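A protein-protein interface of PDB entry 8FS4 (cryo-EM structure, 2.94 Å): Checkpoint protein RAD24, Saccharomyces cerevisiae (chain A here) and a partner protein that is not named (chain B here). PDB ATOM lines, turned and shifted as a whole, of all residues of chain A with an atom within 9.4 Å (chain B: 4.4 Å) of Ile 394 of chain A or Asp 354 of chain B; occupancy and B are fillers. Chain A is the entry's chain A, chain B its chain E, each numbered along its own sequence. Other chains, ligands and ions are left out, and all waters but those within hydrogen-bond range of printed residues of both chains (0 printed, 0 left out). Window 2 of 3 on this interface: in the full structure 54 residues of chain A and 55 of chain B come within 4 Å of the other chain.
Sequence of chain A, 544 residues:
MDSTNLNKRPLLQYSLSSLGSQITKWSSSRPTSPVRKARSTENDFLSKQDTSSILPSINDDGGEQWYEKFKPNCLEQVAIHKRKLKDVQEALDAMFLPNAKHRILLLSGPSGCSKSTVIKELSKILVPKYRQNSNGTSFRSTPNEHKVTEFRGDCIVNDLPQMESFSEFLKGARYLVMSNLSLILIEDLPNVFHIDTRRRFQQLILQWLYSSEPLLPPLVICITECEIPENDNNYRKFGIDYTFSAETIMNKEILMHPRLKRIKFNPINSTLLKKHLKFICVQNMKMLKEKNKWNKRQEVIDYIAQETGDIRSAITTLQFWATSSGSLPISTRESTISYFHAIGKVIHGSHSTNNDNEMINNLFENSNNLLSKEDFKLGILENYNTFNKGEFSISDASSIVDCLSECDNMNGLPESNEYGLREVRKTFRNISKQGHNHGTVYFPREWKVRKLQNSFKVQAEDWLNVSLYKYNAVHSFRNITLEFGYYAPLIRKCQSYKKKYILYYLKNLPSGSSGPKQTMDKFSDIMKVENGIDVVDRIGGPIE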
ATOM      1  N   TYR A 384       6.076   4.524  -3.331  1.00  0.00           N
ATOM      2  CA  TYR A 384       6.325   3.931  -2.025  1.00  0.00           C
ATOM      3  C   TYR A 384       5.039   3.681  -1.248  1.00  0.00           C
ATOM      4  O   TYR A 384       5.074   2.966  -0.242  1.00  0.00           O
ATOM      5  CB  TYR A 384       7.267   4.817  -1.210  1.00  0.00           C
ATOM      6  CG  TYR A 384       6.573   5.920  -0.446  1.00  0.00           C
ATOM      7  CD1 TYR A 384       6.128   7.058  -1.094  1.00  0.00           C
ATOM      8  CD2 TYR A 384       6.372   5.825   0.923  1.00  0.00           C
ATOM      9  CE1 TYR A 384       5.496   8.069  -0.408  1.00  0.00           C
ATOM     10  CE2 TYR A 384       5.741   6.833   1.621  1.00  0.00           C
ATOM     11  CZ  TYR A 384       5.305   7.953   0.948  1.00  0.00           C
ATOM     12  OH  TYR A 384       4.674   8.967   1.626  1.00  0.00           O
ATOM     13  N   GLY A 390      -0.647   0.696   0.752  1.00  0.00           N
ATOM     14  CA  GLY A 390      -0.642   1.912   1.532  1.00  0.00           C
ATOM     15  C   GLY A 390      -1.118   1.745   2.953  1.00  0.00           C
ATOM     16  O   GLY A 390      -1.714   2.675   3.508  1.00  0.00           O
ATOM     17  N   GLU A 391      -0.871   0.589   3.567  1.00  0.00           N
ATOM     18  CA  GLU A 391      -1.371   0.311   4.907  1.00  0.00           C
ATOM     19  C   GLU A 391      -0.223   0.139   5.894  1.00  0.00           C
ATOM     20  O   GLU A 391      -0.261  -0.760   6.739  1.00  0.00           O
ATOM     21  CB  GLU A 391      -2.241  -0.947   4.902  1.00  0.00           C
ATOM     22  CG  GLU A 391      -3.339  -0.951   3.851  1.00  0.00           C
ATOM     23  CD  GLU A 391      -4.429   0.059   4.138  1.00  0.00           C
ATOM     24  OE1 GLU A 391      -4.535   0.511   5.296  1.00  0.00           O
ATOM     25  OE2 GLU A 391      -5.182   0.402   3.203  1.00  0.00           O
ATOM     26  N   PHE A 392       0.795   0.987   5.800  1.00  0.00           N
ATOM     27  CA  PHE A 392       1.945   0.924   6.688  1.00  0.00           C
ATOM     28  C   PHE A 392       2.003   2.180   7.546  1.00  0.00           C
ATOM     29  O   PHE A 392       1.330   3.180   7.282  1.00  0.00           O
ATOM     30  CB  PHE A 392       3.253   0.738   5.903  1.00  0.00           C
ATOM     31  CG  PHE A 392       3.441   1.704   4.768  1.00  0.00           C
ATOM     32  CD1 PHE A 392       2.810   1.502   3.555  1.00  0.00           C
ATOM     33  CD2 PHE A 392       4.272   2.798   4.906  1.00  0.00           C
ATOM     34  CE1 PHE A 392       2.990   2.384   2.512  1.00  0.00           C
ATOM     35  CE2 PHE A 392       4.456   3.680   3.865  1.00  0.00           C
ATOM     36  CZ  PHE A 392       3.814   3.472   2.668  1.00  0.00           C
ATOM     37  N   SER A 393       2.821   2.108   8.594  1.00  0.00           N
ATOM     38  CA  SER A 393       2.889   3.176   9.580  1.00  0.00           C
ATOM     39  C   SER A 393       3.168   4.516   8.912  1.00  0.00           C
ATOM     40  O   SER A 393       3.742   4.587   7.823  1.00  0.00           O
ATOM     41  CB  SER A 393       3.976   2.867  10.610  1.00  0.00           C
ATOM     42  OG  SER A 393       3.922   3.768  11.700  1.00  0.00           O
ATOM     43  N   ILE A 394       2.739   5.591   9.574  1.00  0.00           N
ATOM     44  CA  ILE A 394       3.001   6.923   9.042  1.00  0.00           C
ATOM     45  C   ILE A 394       4.425   7.363   9.353  1.00  0.00           C
ATOM     46  O   ILE A 394       4.988   8.196   8.637  1.00  0.00           O
ATOM     47  CB  ILE A 394       1.974   7.932   9.584  1.00  0.00           C
ATOM     48  CG1 ILE A 394       2.102   9.275   8.859  1.00  0.00           C
ATOM     49  CG2 ILE A 394       2.152   8.133  11.083  1.00  0.00           C
ATOM     50  CD1 ILE A 394       1.861   9.210   7.365  1.00  0.00           C
ATOM     51  N   SER A 395       5.031   6.827  10.414  1.00  0.00           N
ATOM     52  CA  SER A 395       6.415   7.173  10.712  1.00  0.00           C
ATOM     53  C   SER A 395       7.341   6.727   9.589  1.00  0.00           C
ATOM     54  O   SER A 395       8.265   7.455   9.210  1.00  0.00           O
ATOM     55  CB  SER A 395       6.840   6.547  12.039  1.00  0.00           C
ATOM     56  OG  SER A 395       5.816   6.673  13.009  1.00  0.00           O
ATOM     57  N   ASP A 396       7.111   5.532   9.044  1.00  0.00           N
ATOM     58  CA  ASP A 396       7.943   5.047   7.947  1.00  0.00           C
ATOM     59  C   ASP A 396       7.800   5.927   6.712  1.00  0.00           C
ATOM     60  O   ASP A 396       8.796   6.262   6.059  1.00  0.00           O
ATOM     61  CB  ASP A 396       7.578   3.602   7.619  1.00  0.00           C
ATOM     62  CG  ASP A 396       7.782   2.671   8.795  1.00  0.00           C
ATOM     63  OD1 ASP A 396       8.911   2.627   9.328  1.00  0.00           O
ATOM     64  OD2 ASP A 396       6.817   1.985   9.189  1.00  0.00           O
ATOM     65  N   ALA A 397       6.568   6.310   6.374  1.00  0.00           N
ATOM     66  CA  ALA A 397       6.358   7.188   5.228  1.00  0.00           C
ATOM     67  C   ALA A 397       7.026   8.538   5.442  1.00  0.00           C
ATOM     68  O   ALA A 397       7.653   9.087   4.526  1.00  0.00           O
ATOM     69  CB  ALA A 397       4.863   7.364   4.977  1.00  0.00           C
ATOM     70  N   SER A 398       6.901   9.093   6.649  1.00  0.00           N
ATOM     71  CA  SER A 398       7.552  10.364   6.941  1.00  0.00           C
ATOM     72  C   SER A 398       9.061  10.242   6.802  1.00  0.00           C
ATOM     73  O   SER A 398       9.709  11.127   6.237  1.00  0.00           O
ATOM     74  CB  SER A 398       7.188  10.838   8.345  1.00  0.00           C
ATOM     75  OG  SER A 398       7.966  10.169   9.320  1.00  0.00           O
ATOM     76  N   SER A 399       9.639   9.152   7.310  1.00  0.00           N
ATOM     77  CA  SER A 399      11.081   8.963   7.193  1.00  0.00           C
ATOM     78  C   SER A 399      11.503   8.868   5.733  1.00  0.00           C
ATOM     79  O   SER A 399      12.497   9.481   5.324  1.00  0.00           O
ATOM     80  CB  SER A 399      11.509   7.711   7.956  1.00  0.00           C
ATOM     81  OG  SER A 399      11.204   7.824   9.335  1.00  0.00           O
ATOM     82  N   ILE A 400      10.751   8.116   4.928  1.00  0.00           N
ATOM     83  CA  ILE A 400      11.102   7.957   3.520  1.00  0.00           C
ATOM     84  C   ILE A 400      11.078   9.304   2.811  1.00  0.00           C
ATOM     85  O   ILE A 400      12.026   9.674   2.106  1.00  0.00           O
ATOM     86  CB  ILE A 400      10.154   6.948   2.846  1.00  0.00           C
ATOM     87  CG1 ILE A 400      10.498   5.528   3.303  1.00  0.00           C
ATOM     88  CG2 ILE A 400      10.223   7.075   1.325  1.00  0.00           C
ATOM     89  CD1 ILE A 400       9.567   4.461   2.778  1.00  0.00           C
ATOM     90  N   VAL A 401       9.991  10.061   2.983  1.00  0.00           N
ATOM     91  CA  VAL A 401       9.876  11.323   2.257  1.00  0.00           C
ATOM     92  C   VAL A 401      10.878  12.343   2.782  1.00  0.00           C
ATOM     93  O   VAL A 401      11.416  13.144   2.007  1.00  0.00           O
ATOM     94  CB  VAL A 401       8.436  11.863   2.317  1.00  0.00           C
ATOM     95  CG1 VAL A 401       8.307  13.092   1.444  1.00  0.00           C
ATOM     96  CG2 VAL A 401       7.453  10.807   1.850  1.00  0.00           C
ATOM     97  N   ASP A 402      11.146  12.349   4.088  1.00  0.00           N
ATOM     98  CA  ASP A 402      12.153  13.253   4.627  1.00  0.00           C
ATOM     99  C   ASP A 402      13.523  12.946   4.047  1.00  0.00           C
ATOM    100  O   ASP A 402      14.274  13.861   3.693  1.00  0.00           O
ATOM    101  CB  ASP A 402      12.184  13.151   6.151  1.00  0.00           C
ATOM    102  CG  ASP A 402      13.419  13.787   6.750  1.00  0.00           C
ATOM    103  OD1 ASP A 402      14.457  13.099   6.846  1.00  0.00           O
ATOM    104  OD2 ASP A 402      13.353  14.974   7.129  1.00  0.00           O
ATOM    105  N   THR A 427      13.783   0.825   5.291  1.00  0.00           N
ATOM    106  CA  THR A 427      12.472   1.099   5.864  1.00  0.00           C
ATOM    107  C   THR A 427      11.469   0.027   5.464  1.00  0.00           C
ATOM    108  O   THR A 427      10.726  -0.485   6.307  1.00  0.00           O
ATOM    109  CB  THR A 427      11.994   2.481   5.415  1.00  0.00           C
ATOM    110  OG1 THR A 427      12.801   3.491   6.032  1.00  0.00           O
ATOM    111  CG2 THR A 427      10.539   2.706   5.790  1.00  0.00           C
ATOM    112  N   ILE A 431       9.563  -3.325   7.933  1.00  0.00           N
ATOM    113  CA  ILE A 431       8.114  -3.430   8.067  1.00  0.00           C
ATOM    114  C   ILE A 431       7.531  -4.578   7.253  1.00  0.00           C
ATOM    115  O   ILE A 431       6.383  -4.970   7.493  1.00  0.00           O
ATOM    116  CB  ILE A 431       7.433  -2.106   7.670  1.00  0.00           C
ATOM    117  CG1 ILE A 431       7.425  -1.916   6.151  1.00  0.00           C
ATOM    118  CG2 ILE A 431       8.128  -0.933   8.346  1.00  0.00           C
ATOM    119  CD1 ILE A 431       6.689  -0.677   5.699  1.00  0.00           C
ATOM    120  N   ARG B 274      -4.938  11.439   9.261  1.00  0.00           N
ATOM    121  CA  ARG B 274      -3.479  11.333   9.279  1.00  0.00           C
ATOM    122  C   ARG B 274      -3.111   9.894   8.930  1.00  0.00           C
ATOM    123  O   ARG B 274      -2.911   9.062   9.819  1.00  0.00           O
ATOM    124  CB  ARG B 274      -2.922  11.747  10.629  1.00  0.00           C
ATOM    125  CG  ARG B 274      -3.250  13.175  11.017  1.00  0.00           C
ATOM    126  CD  ARG B 274      -2.944  13.432  12.479  1.00  0.00           C
ATOM    127  NE  ARG B 274      -3.729  12.574  13.357  1.00  0.00           N
ATOM    128  CZ  ARG B 274      -4.962  12.841  13.763  1.00  0.00           C
ATOM    129  NH1 ARG B 274      -5.590  13.946  13.391  1.00  0.00           N
ATOM    130  NH2 ARG B 274      -5.582  11.978  14.562  1.00  0.00           N
ATOM    131  N   SER B 275      -3.006   9.609   7.636  1.00  0.00           N
ATOM    132  CA  SER B 275      -2.743   8.257   7.164  1.00  0.00           C
ATOM    133  C   SER B 275      -2.125   8.345   5.776  1.00  0.00           C
ATOM    134  O   SER B 275      -2.169   9.386   5.119  1.00  0.00           O
ATOM    135  CB  SER B 275      -4.022   7.418   7.139  1.00  0.00           C
ATOM    136  OG  SER B 275      -4.970   7.965   6.240  1.00  0.00           O
ATOM    137  N   LEU B 279      -2.150  11.122   2.942  1.00  0.00           N
ATOM    138  CA  LEU B 279      -0.932  11.730   2.418  1.00  0.00           C
ATOM    139  C   LEU B 279      -0.949  11.767   0.896  1.00  0.00           C
ATOM    140  O   LEU B 279      -0.531  12.756   0.285  1.00  0.00           O
ATOM    141  CB  LEU B 279       0.283  10.958   2.927  1.00  0.00           C
ATOM    142  CG  LEU B 279       1.638  11.656   2.864  1.00  0.00           C
ATOM    143  CD1 LEU B 279       2.450  11.324   4.100  1.00  0.00           C
ATOM    144  CD2 LEU B 279       2.387  11.244   1.613  1.00  0.00           C
ATOM    145  N   MET B 350       1.728  15.449   9.956  1.00  0.00           N
ATOM    146  CA  MET B 350       0.761  14.457  10.416  1.00  0.00           C
ATOM    147  C   MET B 350       1.416  13.303  11.158  1.00  0.00           C
ATOM    148  O   MET B 350       0.709  12.527  11.808  1.00  0.00           O
ATOM    149  CB  MET B 350      -0.099  13.894   9.275  1.00  0.00           C
ATOM    150  CG  MET B 350       0.505  13.857   7.903  1.00  0.00           C
ATOM    151  SD  MET B 350      -0.725  13.421   6.663  1.00  0.00           S
ATOM    152  CE  MET B 350      -0.506  11.653   6.589  1.00  0.00           C
ATOM    153  N   CYS B 351       2.739  13.165  11.085  1.00  0.00           N
ATOM    154  CA  CYS B 351       3.430  12.264  11.994  1.00  0.00           C
ATOM    155  C   CYS B 351       3.586  12.864  13.383  1.00  0.00           C
ATOM    156  O   CYS B 351       3.781  12.119  14.347  1.00  0.00           O
ATOM    157  CB  CYS B 351       4.806  11.902  11.433  1.00  0.00           C
ATOM    158  SG  CYS B 351       5.630  10.564  12.319  1.00  0.00           S
ATOM    159  N   CYS B 352       3.513  14.189  13.501  1.00  0.00           N
ATOM    160  CA  CYS B 352       3.608  14.842  14.801  1.00  0.00           C
ATOM    161  C   CYS B 352       2.248  15.014  15.470  1.00  0.00           C
ATOM    162  O   CYS B 352       2.149  14.906  16.696  1.00  0.00           O
ATOM    163  CB  CYS B 352       4.284  16.208  14.659  1.00  0.00           C
ATOM    164  SG  CYS B 352       3.146  17.609  14.674  1.00  0.00           S
ATOM    165  N   LEU B 353       1.192  15.280  14.695  1.00  0.00           N
ATOM    166  CA  LEU B 353      -0.114  15.509  15.309  1.00  0.00           C
ATOM    167  C   LEU B 353      -0.703  14.234  15.898  1.00  0.00           C
ATOM    168  O   LEU B 353      -1.549  14.306  16.796  1.00  0.00           O
ATOM    169  CB  LEU B 353      -1.091  16.103  14.295  1.00  0.00           C
ATOM    170  CG  LEU B 353      -0.653  17.366  13.558  1.00  0.00           C
ATOM    171  CD1 LEU B 353      -1.408  17.499  12.250  1.00  0.00           C
ATOM    172  CD2 LEU B 353      -0.863  18.590  14.422  1.00  0.00           C
ATOM    173  N   ASP B 354      -0.283  13.069  15.417  1.00  0.00           N
ATOM    174  CA  ASP B 354      -0.863  11.806  15.866  1.00  0.00           C
ATOM    175  C   ASP B 354      -0.450  11.465  17.294  1.00  0.00           C
ATOM    176  O   ASP B 354      -1.065  10.615  17.940  1.00  0.00           O
ATOM    177  CB  ASP B 354      -0.465  10.669  14.924  1.00  0.00           C
ATOM    178  CG  ASP B 354       0.966  10.215  15.126  1.00  0.00           C
ATOM    179  OD1 ASP B 354       1.795  11.031  15.576  1.00  0.00           O
ATOM    180  OD2 ASP B 354       1.264   9.040  14.826  1.00  0.00           O
ATOM    181  OXT ASP B 354       0.504  12.022  17.835  1.00  0.00           O
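The backbone carbonyl oxygen (O) of Cys 351 of chain B sits close to the side-chain carboxylate (OD1) of Asp 354 of chain B (2.6 Å). N of Ser 395 of chain A sits close to OG of Ser 393 of chain A, at 3.5 Å. O of Ser 395 of chain A lies within hydrogen-bond range of OG of Ser 398 of chain A (2.7 Å). OG of Ser 399 of chain A sits at hydrogen-bond distance from O of Ser 395 of chain A.
CD2 of Leu 279 of chain B touches OH of Tyr 384 of chain A, 3.2 Å away. Ile 394 of chain A touches Leu 279 of chain B. CD1 of Ile 394 of chain A touches CE of Met 350 of chain B, at 3.5 Å. Ile 394 of chain A touches Asp 354 of chain B (CG2 to OD2, 3.95 Å). Ser 395 of chain A touches Cys 351 of chain B. Ser 398 of chain A touches Cys 351 of chain B.
Of the printed residues of chain B, Tyr 384 of chain A touches Leu 279 (3.2 Å). Ile 394 of chain A touches three residues of chain B. Of the printed residues of chain B, Ser 395 of chain A touches Cys 351. Printed residues of chain B within 4 Å of Ser 398 of chain A: Cys 351 (3.8 Å). Arg 274 of chain B touches none of the printed residues of chain A. Ser 275 of chain B touches none of the printed residues of chain A. Of the printed residues of chain A, Met 350 of chain B touches Ile 394 (3.5 Å). Cys 351 of chain B touches just these residues of chain A: Ser 395 and Ser 398. Asp 354 of chain B touches just one residue of chain A: Ile 394 (3.95 Å).
Printed residues of chain B that touch a printed residue of chain A: Leu 279, Met 350, Cys 351 and Asp 354. Hydrophobic or aromatic side chains of chain B that line the printed part of chain A: Leu 279 and Met 350. Hydrophobic or aromatic side chains of chain A within 4 Å of the printed part of chain B: Tyr 384 and Ile 394. Among the printed residues, 6 pairs touch across the chains. Among the printed residues, no Asp or Glu carboxylate lies within 4 Å of a Lys or Arg side-chain nitrogen of the other chain.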
